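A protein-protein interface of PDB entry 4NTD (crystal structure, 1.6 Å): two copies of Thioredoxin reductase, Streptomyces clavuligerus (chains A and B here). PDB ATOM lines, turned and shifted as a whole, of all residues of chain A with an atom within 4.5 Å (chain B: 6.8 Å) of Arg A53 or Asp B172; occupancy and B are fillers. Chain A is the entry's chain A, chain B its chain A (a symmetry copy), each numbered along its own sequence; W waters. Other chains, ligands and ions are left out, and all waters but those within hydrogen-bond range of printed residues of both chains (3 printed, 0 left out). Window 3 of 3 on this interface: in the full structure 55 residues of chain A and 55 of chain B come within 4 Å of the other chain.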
ATOM      1  N   LEU A  49      27.616  -4.918  -4.138  1.00  0.00           N
ATOM      2  CA  LEU A  49      27.119  -5.502  -2.887  1.00  0.00           C
ATOM      3  C   LEU A  49      25.687  -5.078  -2.553  1.00  0.00           C
ATOM      4  O   LEU A  49      24.885  -5.904  -2.113  1.00  0.00           O
ATOM      5  CB  LEU A  49      28.051  -5.165  -1.719  1.00  0.00           C
ATOM      6  CG  LEU A  49      29.416  -5.859  -1.757  1.00  0.00           C
ATOM      7  CD1 LEU A  49      30.385  -5.184  -0.798  1.00  0.00           C
ATOM      8  CD2 LEU A  49      29.285  -7.343  -1.444  1.00  0.00           C
ATOM      9  N   ALA A  50      25.366  -3.802  -2.764  1.00  0.00           N
ATOM     10  CA  ALA A  50      24.007  -3.301  -2.529  1.00  0.00           C
ATOM     11  C   ALA A  50      23.014  -3.908  -3.523  1.00  0.00           C
ATOM     12  O   ALA A  50      21.888  -4.244  -3.154  1.00  0.00           O
ATOM     13  CB  ALA A  50      23.974  -1.781  -2.601  1.00  0.00           C
ATOM     14  N   ARG A  51      23.440  -4.059  -4.776  1.00  0.00           N
ATOM     15  CA  ARG A  51      22.631  -4.744  -5.788  1.00  0.00           C
ATOM     16  C   ARG A  51      22.416  -6.225  -5.441  1.00  0.00           C
ATOM     17  O   ARG A  51      21.422  -6.824  -5.857  1.00  0.00           O
ATOM     18  CB  ARG A  51      23.266  -4.605  -7.176  1.00  0.00           C
ATOM     19  CG  ARG A  51      23.070  -3.230  -7.811  1.00  0.00           C
ATOM     20  CD  ARG A  51      23.730  -3.137  -9.180  1.00  0.00           C
ATOM     21  NE  ARG A  51      23.398  -4.309  -9.982  1.00  0.00           N
ATOM     22  CZ  ARG A  51      22.234  -4.512 -10.598  1.00  0.00           C
ATOM     23  NH1 ARG A  51      21.269  -3.597 -10.565  1.00  0.00           N
ATOM     24  NH2 ARG A  51      22.041  -5.639 -11.272  1.00  0.00           N
ATOM     25  N   ALA A  52      23.344  -6.799  -4.673  1.00  0.00           N
ATOM     26  CA  ALA A  52      23.211  -8.162  -4.144  1.00  0.00           C
ATOM     27  C   ALA A  52      22.391  -8.230  -2.844  1.00  0.00           C
ATOM     28  O   ALA A  52      22.375  -9.265  -2.172  1.00  0.00           O
ATOM     29  CB  ALA A  52      24.588  -8.778  -3.939  1.00  0.00           C
ATOM     30  N   ARG A  53      21.728  -7.119  -2.512  1.00  0.00           N
ATOM     31  CA  ARG A  53      20.836  -7.027  -1.352  1.00  0.00           C
ATOM     32  C   ARG A  53      21.561  -7.218  -0.015  1.00  0.00           C
ATOM     33  O   ARG A  53      20.953  -7.623   0.976  1.00  0.00           O
ATOM     34  CB  ARG A  53      19.662  -8.010  -1.483  1.00  0.00           C
ATOM     35  CG  ARG A  53      18.963  -7.950  -2.833  1.00  0.00           C
ATOM     36  CD  ARG A  53      17.636  -8.692  -2.819  1.00  0.00           C
ATOM     37  NE  ARG A  53      16.592  -7.933  -2.136  1.00  0.00           N
ATOM     38  CZ  ARG A  53      15.400  -8.426  -1.819  1.00  0.00           C
ATOM     39  NH1 ARG A  53      15.100  -9.683  -2.116  1.00  0.00           N
ATOM     40  NH2 ARG A  53      14.507  -7.665  -1.201  1.00  0.00           N
ATOM     41  N   ARG A  54      22.857  -6.913   0.010  1.00  0.00           N
ATOM     42  CA  ARG A  54      23.621  -6.904   1.253  1.00  0.00           C
ATOM     43  C   ARG A  54      23.495  -5.512   1.856  1.00  0.00           C
ATOM     44  O   ARG A  54      23.453  -4.520   1.125  1.00  0.00           O
ATOM     45  CB  ARG A  54      25.093  -7.234   1.006  1.00  0.00           C
ATOM     46  CG  ARG A  54      25.339  -8.610   0.407  1.00  0.00           C
ATOM     47  CD  ARG A  54      24.910  -9.726   1.346  1.00  0.00           C
ATOM     48  NE  ARG A  54      25.217 -11.040   0.788  1.00  0.00           N
ATOM     49  CZ  ARG A  54      24.916 -12.203   1.362  1.00  0.00           C
ATOM     50  NH1 ARG A  54      24.289 -12.246   2.535  1.00  0.00           N
ATOM     51  NH2 ARG A  54      25.246 -13.336   0.753  1.00  0.00           N
ATOM     52  N   ARG A  55      23.424  -5.447   3.184  1.00  0.00           N
ATOM     53  CA  ARG A  55      23.342  -4.173   3.885  1.00  0.00           C
ATOM     54  C   ARG A  55      24.743  -3.581   4.030  1.00  0.00           C
ATOM     55  O   ARG A  55      25.593  -4.136   4.732  1.00  0.00           O
ATOM     56  CB  ARG A  55      22.657  -4.357   5.239  1.00  0.00           C
ATOM     57  CG  ARG A  55      21.241  -4.890   5.089  1.00  0.00           C
ATOM     58  CD  ARG A  55      20.522  -4.147   3.974  1.00  0.00           C
ATOM     59  NE  ARG A  55      19.705  -5.027   3.142  1.00  0.00           N
ATOM     60  CZ  ARG A  55      19.374  -4.757   1.884  1.00  0.00           C
ATOM     61  NH1 ARG A  55      19.798  -3.637   1.318  1.00  0.00           N
ATOM     62  NH2 ARG A  55      18.628  -5.603   1.189  1.00  0.00           N
ATOM     63  N   GLY B 167      20.170 -10.092 -10.865  1.00  0.00           N
ATOM     64  CA  GLY B 167      19.489 -10.461  -9.627  1.00  0.00           C
ATOM     65  C   GLY B 167      18.605  -9.366  -9.068  1.00  0.00           C
ATOM     66  O   GLY B 167      17.438  -9.602  -8.758  1.00  0.00           O
ATOM     67  N   TYR B 168      19.154  -8.164  -8.935  1.00  0.00           N
ATOM     68  CA  TYR B 168      18.391  -7.058  -8.367  1.00  0.00           C
ATOM     69  C   TYR B 168      17.083  -6.833  -9.127  1.00  0.00           C
ATOM     70  O   TYR B 168      16.030  -6.620  -8.519  1.00  0.00           O
ATOM     71  CB  TYR B 168      19.207  -5.765  -8.359  1.00  0.00           C
ATOM     72  CG  TYR B 168      18.448  -4.639  -7.709  1.00  0.00           C
ATOM     73  CD1 TYR B 168      18.456  -4.484  -6.329  1.00  0.00           C
ATOM     74  CD2 TYR B 168      17.680  -3.761  -8.468  1.00  0.00           C
ATOM     75  CE1 TYR B 168      17.741  -3.468  -5.720  1.00  0.00           C
ATOM     76  CE2 TYR B 168      16.959  -2.743  -7.869  1.00  0.00           C
ATOM     77  CZ  TYR B 168      16.996  -2.601  -6.497  1.00  0.00           C
ATOM     78  OH  TYR B 168      16.288  -1.591  -5.894  1.00  0.00           O
ATOM     79  N   VAL B 170      15.211  -8.851 -10.693  1.00  0.00           N
ATOM     80  CA  VAL B 170      14.201  -9.894 -10.479  1.00  0.00           C
ATOM     81  C   VAL B 170      14.044 -10.251  -8.993  1.00  0.00           C
ATOM     82  O   VAL B 170      13.623 -11.359  -8.655  1.00  0.00           O
ATOM     83  CB  VAL B 170      14.494 -11.153 -11.330  1.00  0.00           C
ATOM     84  CG1 VAL B 170      14.497 -10.794 -12.810  1.00  0.00           C
ATOM     85  CG2 VAL B 170      15.811 -11.810 -10.937  1.00  0.00           C
ATOM     86  N   SER B 171      14.358  -9.294  -8.119  1.00  0.00           N
ATOM     87  CA  SER B 171      14.242  -9.477  -6.672  1.00  0.00           C
ATOM     88  C   SER B 171      12.857  -9.981  -6.277  1.00  0.00           C
ATOM     89  O   SER B 171      11.847  -9.464  -6.753  1.00  0.00           O
ATOM     90  CB  SER B 171      14.510  -8.157  -5.937  1.00  0.00           C
ATOM     91  OG  SER B 171      15.859  -7.749  -6.065  1.00  0.00           O
ATOM     92  N   ASP B 172      12.828 -11.000  -5.418  1.00  0.00           N
ATOM     93  CA  ASP B 172      11.589 -11.543  -4.843  1.00  0.00           C
ATOM     94  C   ASP B 172      10.638 -12.216  -5.844  1.00  0.00           C
ATOM     95  O   ASP B 172       9.509 -12.556  -5.483  1.00  0.00           O
ATOM     96  CB  ASP B 172      10.828 -10.457  -4.064  1.00  0.00           C
ATOM     97  CG  ASP B 172      11.689  -9.776  -3.018  1.00  0.00           C
ATOM     98  OD1 ASP B 172      12.374 -10.483  -2.252  1.00  0.00           O
ATOM     99  OD2 ASP B 172      11.680  -8.528  -2.954  1.00  0.00           O
ATOM    100  N   GLN B 173      11.080 -12.421  -7.083  1.00  0.00           N
ATOM    101  CA  GLN B 173      10.238 -13.065  -8.092  1.00  0.00           C
ATOM    102  C   GLN B 173      10.402 -14.586  -8.045  1.00  0.00           C
ATOM    103  O   GLN B 173      11.347 -15.089  -7.438  1.00  0.00           O
ATOM    104  CB  GLN B 173      10.569 -12.544  -9.489  1.00  0.00           C
ATOM    105  CG  GLN B 173      10.257 -11.067  -9.680  1.00  0.00           C
ATOM    106  CD  GLN B 173      10.454 -10.599 -11.110  1.00  0.00           C
ATOM    107  OE1 GLN B 173      10.443 -11.397 -12.049  1.00  0.00           O
ATOM    108  NE2 GLN B 173      10.630  -9.291 -11.284  1.00  0.00           N
ATOM    109  N   PRO B 174       9.471 -15.328  -8.678  1.00  0.00           N
ATOM    110  CA  PRO B 174       9.626 -16.783  -8.758  1.00  0.00           C
ATOM    111  C   PRO B 174      10.714 -17.176  -9.759  1.00  0.00           C
ATOM    112  O   PRO B 174      10.500 -17.109 -10.974  1.00  0.00           O
ATOM    113  CB  PRO B 174       8.237 -17.274  -9.207  1.00  0.00           C
ATOM    114  CG  PRO B 174       7.322 -16.105  -9.061  1.00  0.00           C
ATOM    115  CD  PRO B 174       8.175 -14.889  -9.225  1.00  0.00           C
ATOM    116  N   LEU B 175      11.874 -17.570  -9.238  1.00  0.00           N
ATOM    117  CA  LEU B 175      13.040 -17.888 -10.060  1.00  0.00           C
ATOM    118  C   LEU B 175      13.221 -19.394 -10.191  1.00  0.00           C
ATOM    119  O   LEU B 175      12.965 -20.142  -9.247  1.00  0.00           O
ATOM    120  CB  LEU B 175      14.309 -17.289  -9.448  1.00  0.00           C
ATOM    121  CG  LEU B 175      14.248 -15.832  -8.987  1.00  0.00           C
ATOM    122  CD1 LEU B 175      15.608 -15.393  -8.469  1.00  0.00           C
ATOM    123  CD2 LEU B 175      13.773 -14.914 -10.104  1.00  0.00           C
ATOM    124  N   ARG B 192      19.195 -17.566  -4.038  1.00  0.00           N
ATOM    125  CA  ARG B 192      18.381 -17.378  -2.828  1.00  0.00           C
ATOM    126  C   ARG B 192      18.685 -16.070  -2.096  1.00  0.00           C
ATOM    127  O   ARG B 192      17.889 -15.622  -1.271  1.00  0.00           O
ATOM    128  CB  ARG B 192      18.528 -18.562  -1.860  1.00  0.00           C
ATOM    129  CG  ARG B 192      17.537 -19.685  -2.108  1.00  0.00           C
ATOM    130  CD  ARG B 192      16.121 -19.315  -1.678  1.00  0.00           C
ATOM    131  NE  ARG B 192      15.907 -19.405  -0.230  1.00  0.00           N
ATOM    132  CZ  ARG B 192      15.828 -18.379   0.622  1.00  0.00           C
ATOM    133  NH1 ARG B 192      15.956 -17.117   0.217  1.00  0.00           N
ATOM    134  NH2 ARG B 192      15.619 -18.622   1.912  1.00  0.00           N
ATOM    135  N   GLN B 193      19.834 -15.466  -2.392  1.00  0.00           N
ATOM    136  CA  GLN B 193      20.163 -14.142  -1.874  1.00  0.00           C
ATOM    137  C   GLN B 193      19.261 -13.042  -2.468  1.00  0.00           C
ATOM    138  O   GLN B 193      19.103 -11.982  -1.863  1.00  0.00           O
ATOM    139  CB  GLN B 193      21.652 -13.844  -2.119  1.00  0.00           C
ATOM    140  CG  GLN B 193      22.146 -12.481  -1.656  1.00  0.00           C
ATOM    141  CD  GLN B 193      21.854 -12.190  -0.193  1.00  0.00           C
ATOM    142  OE1 GLN B 193      21.708 -13.103   0.620  1.00  0.00           O
ATOM    143  NE2 GLN B 193      21.778 -10.909   0.148  1.00  0.00           N
ATOM    144  N   TRP B 194      18.659 -13.304  -3.631  1.00  0.00           N
ATOM    145  CA  TRP B 194      17.781 -12.331  -4.297  1.00  0.00           C
ATOM    146  C   TRP B 194      16.275 -12.628  -4.208  1.00  0.00           C
ATOM    147  O   TRP B 194      15.462 -11.734  -4.439  1.00  0.00           O
ATOM    148  CB  TRP B 194      18.178 -12.191  -5.769  1.00  0.00           C
ATOM    149  CG  TRP B 194      19.418 -11.374  -5.992  1.00  0.00           C
ATOM    150  CD1 TRP B 194      19.482 -10.027  -6.202  1.00  0.00           C
ATOM    151  CD2 TRP B 194      20.768 -11.851  -6.039  1.00  0.00           C
ATOM    152  NE1 TRP B 194      20.788  -9.635  -6.380  1.00  0.00           N
ATOM    153  CE2 TRP B 194      21.598 -10.736  -6.281  1.00  0.00           C
ATOM    154  CE3 TRP B 194      21.358 -13.113  -5.894  1.00  0.00           C
ATOM    155  CZ2 TRP B 194      22.989 -10.845  -6.389  1.00  0.00           C
ATOM    156  CZ3 TRP B 194      22.740 -13.220  -5.997  1.00  0.00           C
ATOM    157  CH2 TRP B 194      23.539 -12.091  -6.241  1.00  0.00           C
ATOM    158  N   SER B 195      15.899 -13.867  -3.893  1.00  0.00           N
ATOM    159  CA  SER B 195      14.481 -14.227  -3.756  1.00  0.00           C
ATOM    160  C   SER B 195      14.299 -15.408  -2.813  1.00  0.00           C
ATOM    161  O   SER B 195      15.166 -16.273  -2.739  1.00  0.00           O
ATOM    162  CB  SER B 195      13.887 -14.583  -5.124  1.00  0.00           C
ATOM    163  OG  SER B 195      12.509 -14.905  -5.019  1.00  0.00           O
ATOM    164  N   ASP B 196      13.165 -15.440  -2.107  1.00  0.00           N
ATOM    165  CA  ASP B 196      12.861 -16.595  -1.256  1.00  0.00           C
ATOM    166  C   ASP B 196      12.078 -17.665  -2.021  1.00  0.00           C
ATOM    167  O   ASP B 196      11.732 -18.701  -1.460  1.00  0.00           O
ATOM    168  CB  ASP B 196      12.152 -16.187   0.048  1.00  0.00           C
ATOM    169  CG  ASP B 196      10.778 -15.590  -0.178  1.00  0.00           C
ATOM    170  OD1 ASP B 196      10.320 -15.550  -1.336  1.00  0.00           O
ATOM    171  OD2 ASP B 196      10.155 -15.152   0.813  1.00  0.00           O
ATOM    172  N   ASP B 197      11.841 -17.420  -3.314  1.00  0.00           N
ATOM    173  CA  ASP B 197      11.132 -18.351  -4.193  1.00  0.00           C
ATOM    174  C   ASP B 197      12.065 -18.777  -5.332  1.00  0.00           C
ATOM    175  O   ASP B 197      12.059 -18.187  -6.416  1.00  0.00           O
ATOM    176  CB  ASP B 197       9.865 -17.670  -4.734  1.00  0.00           C
ATOM    177  CG  ASP B 197       8.935 -18.623  -5.474  1.00  0.00           C
ATOM    178  OD1 ASP B 197       9.288 -19.803  -5.689  1.00  0.00           O
ATOM    179  OD2 ASP B 197       7.830 -18.179  -5.843  1.00  0.00           O
HETATM  180  O   HOH W   1      22.213  -8.044  -8.735  1.00  0.00           O
HETATM  181  O   HOH W   2      15.381  -5.627  -4.041  1.00  0.00           O
HETATM  182  O   HOH W   3      20.007  -9.746   2.630  1.00  0.00           O
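Among the printed residues, merely in contact across the chains: Arg A51 with Tyr B168 (3.5 Å), Ala A52 with Trp B194 (3.5 Å) and Arg A53 with Ser B171 (3.8 Å).
O of Arg A51 sits at hydrogen-bond distance from NE1 of Trp B194 (2.9 Å).
The backbone carbonyl oxygen (O) of Ala A52 lies within hydrogen-bond range of the side-chain amide nitrogen (NE2) of Gln B193 (2.9 Å).
NH1 of Arg A53 lies within salt-bridge range of OD1 of Asp B172 (2.8 Å).
The backbone carbonyl oxygen (O) of Arg A53 is in hydrogen-bond range of the side-chain amide nitrogen (NE2) of Gln B193 (3.5 Å).
NH1 of Arg A53 sits at hydrogen-bond distance from O of Trp B194, 3.1 Å away.
NH1 of Arg A54 is in hydrogen-bond range of OE1 of Gln B193 (3.3 Å).
Printed residues of chain B within 4 Å of Arg A51: Tyr B168 and Trp B194.
Printed residues of chain B within 4 Å of Arg A53: Ser B171, Asp B172, Gln B193 and Trp B194.
Printed residues of chain B within 4 Å of Arg A54: Gln B193 (3.3 Å).
Printed residues of chain A within 4 Å of Asp B172: Arg A53.
Printed residues of chain A within 4 Å of Gln B193: Ala A52 (2.9 Å), Arg A53 (3.5 Å) and Arg A54 (3.3 Å).
The nearest printed residue of chain A that does not touch Asp B172 is Arg A55 (8.6 Å).
No position is printed for both chains.
Hydrophobic or aromatic side chains of chain B within 4 Å of the printed part of chain A: Tyr B168 and Trp B194.
Hydrophobic or aromatic side chains of chain A that line the printed part of chain B: Ala A52.
Along chain A the printed residues that touch a printed residue of chain B span positions 51 to 54.
O of Leu A49 lies within hydrogen-bond range of N of Arg A54, at 3.1 Å.
O of Arg A53 is in hydrogen-bond range of NH2 of Arg A55 (3.1 Å).
The backbone carbonyl oxygen (O) of Tyr B168 sits at hydrogen-bond distance from the side-chain hydroxyl (OG) of Ser B171 (2.7 Å).
N of Asp B172 lies within hydrogen-bond range of O of Trp B194.
Water W3 lies within hydrogen-bond range of the backbone carbonyl oxygen of Arg A53 (2.9 Å) and the side-chain amide nitrogen of Gln B193 (3.3 Å).
Water W2 bridges OG of Ser B171 (3.0 Å) and NE of Arg A53 (3.2 Å).
Water W1 lies within hydrogen-bond range of the backbone NH (N) of Tyr B168 (3.1 Å), the indole nitrogen (NE1) of Trp B194 (3.2 Å) and the backbone carbonyl oxygen (O) of Arg A51 (3.2 Å).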
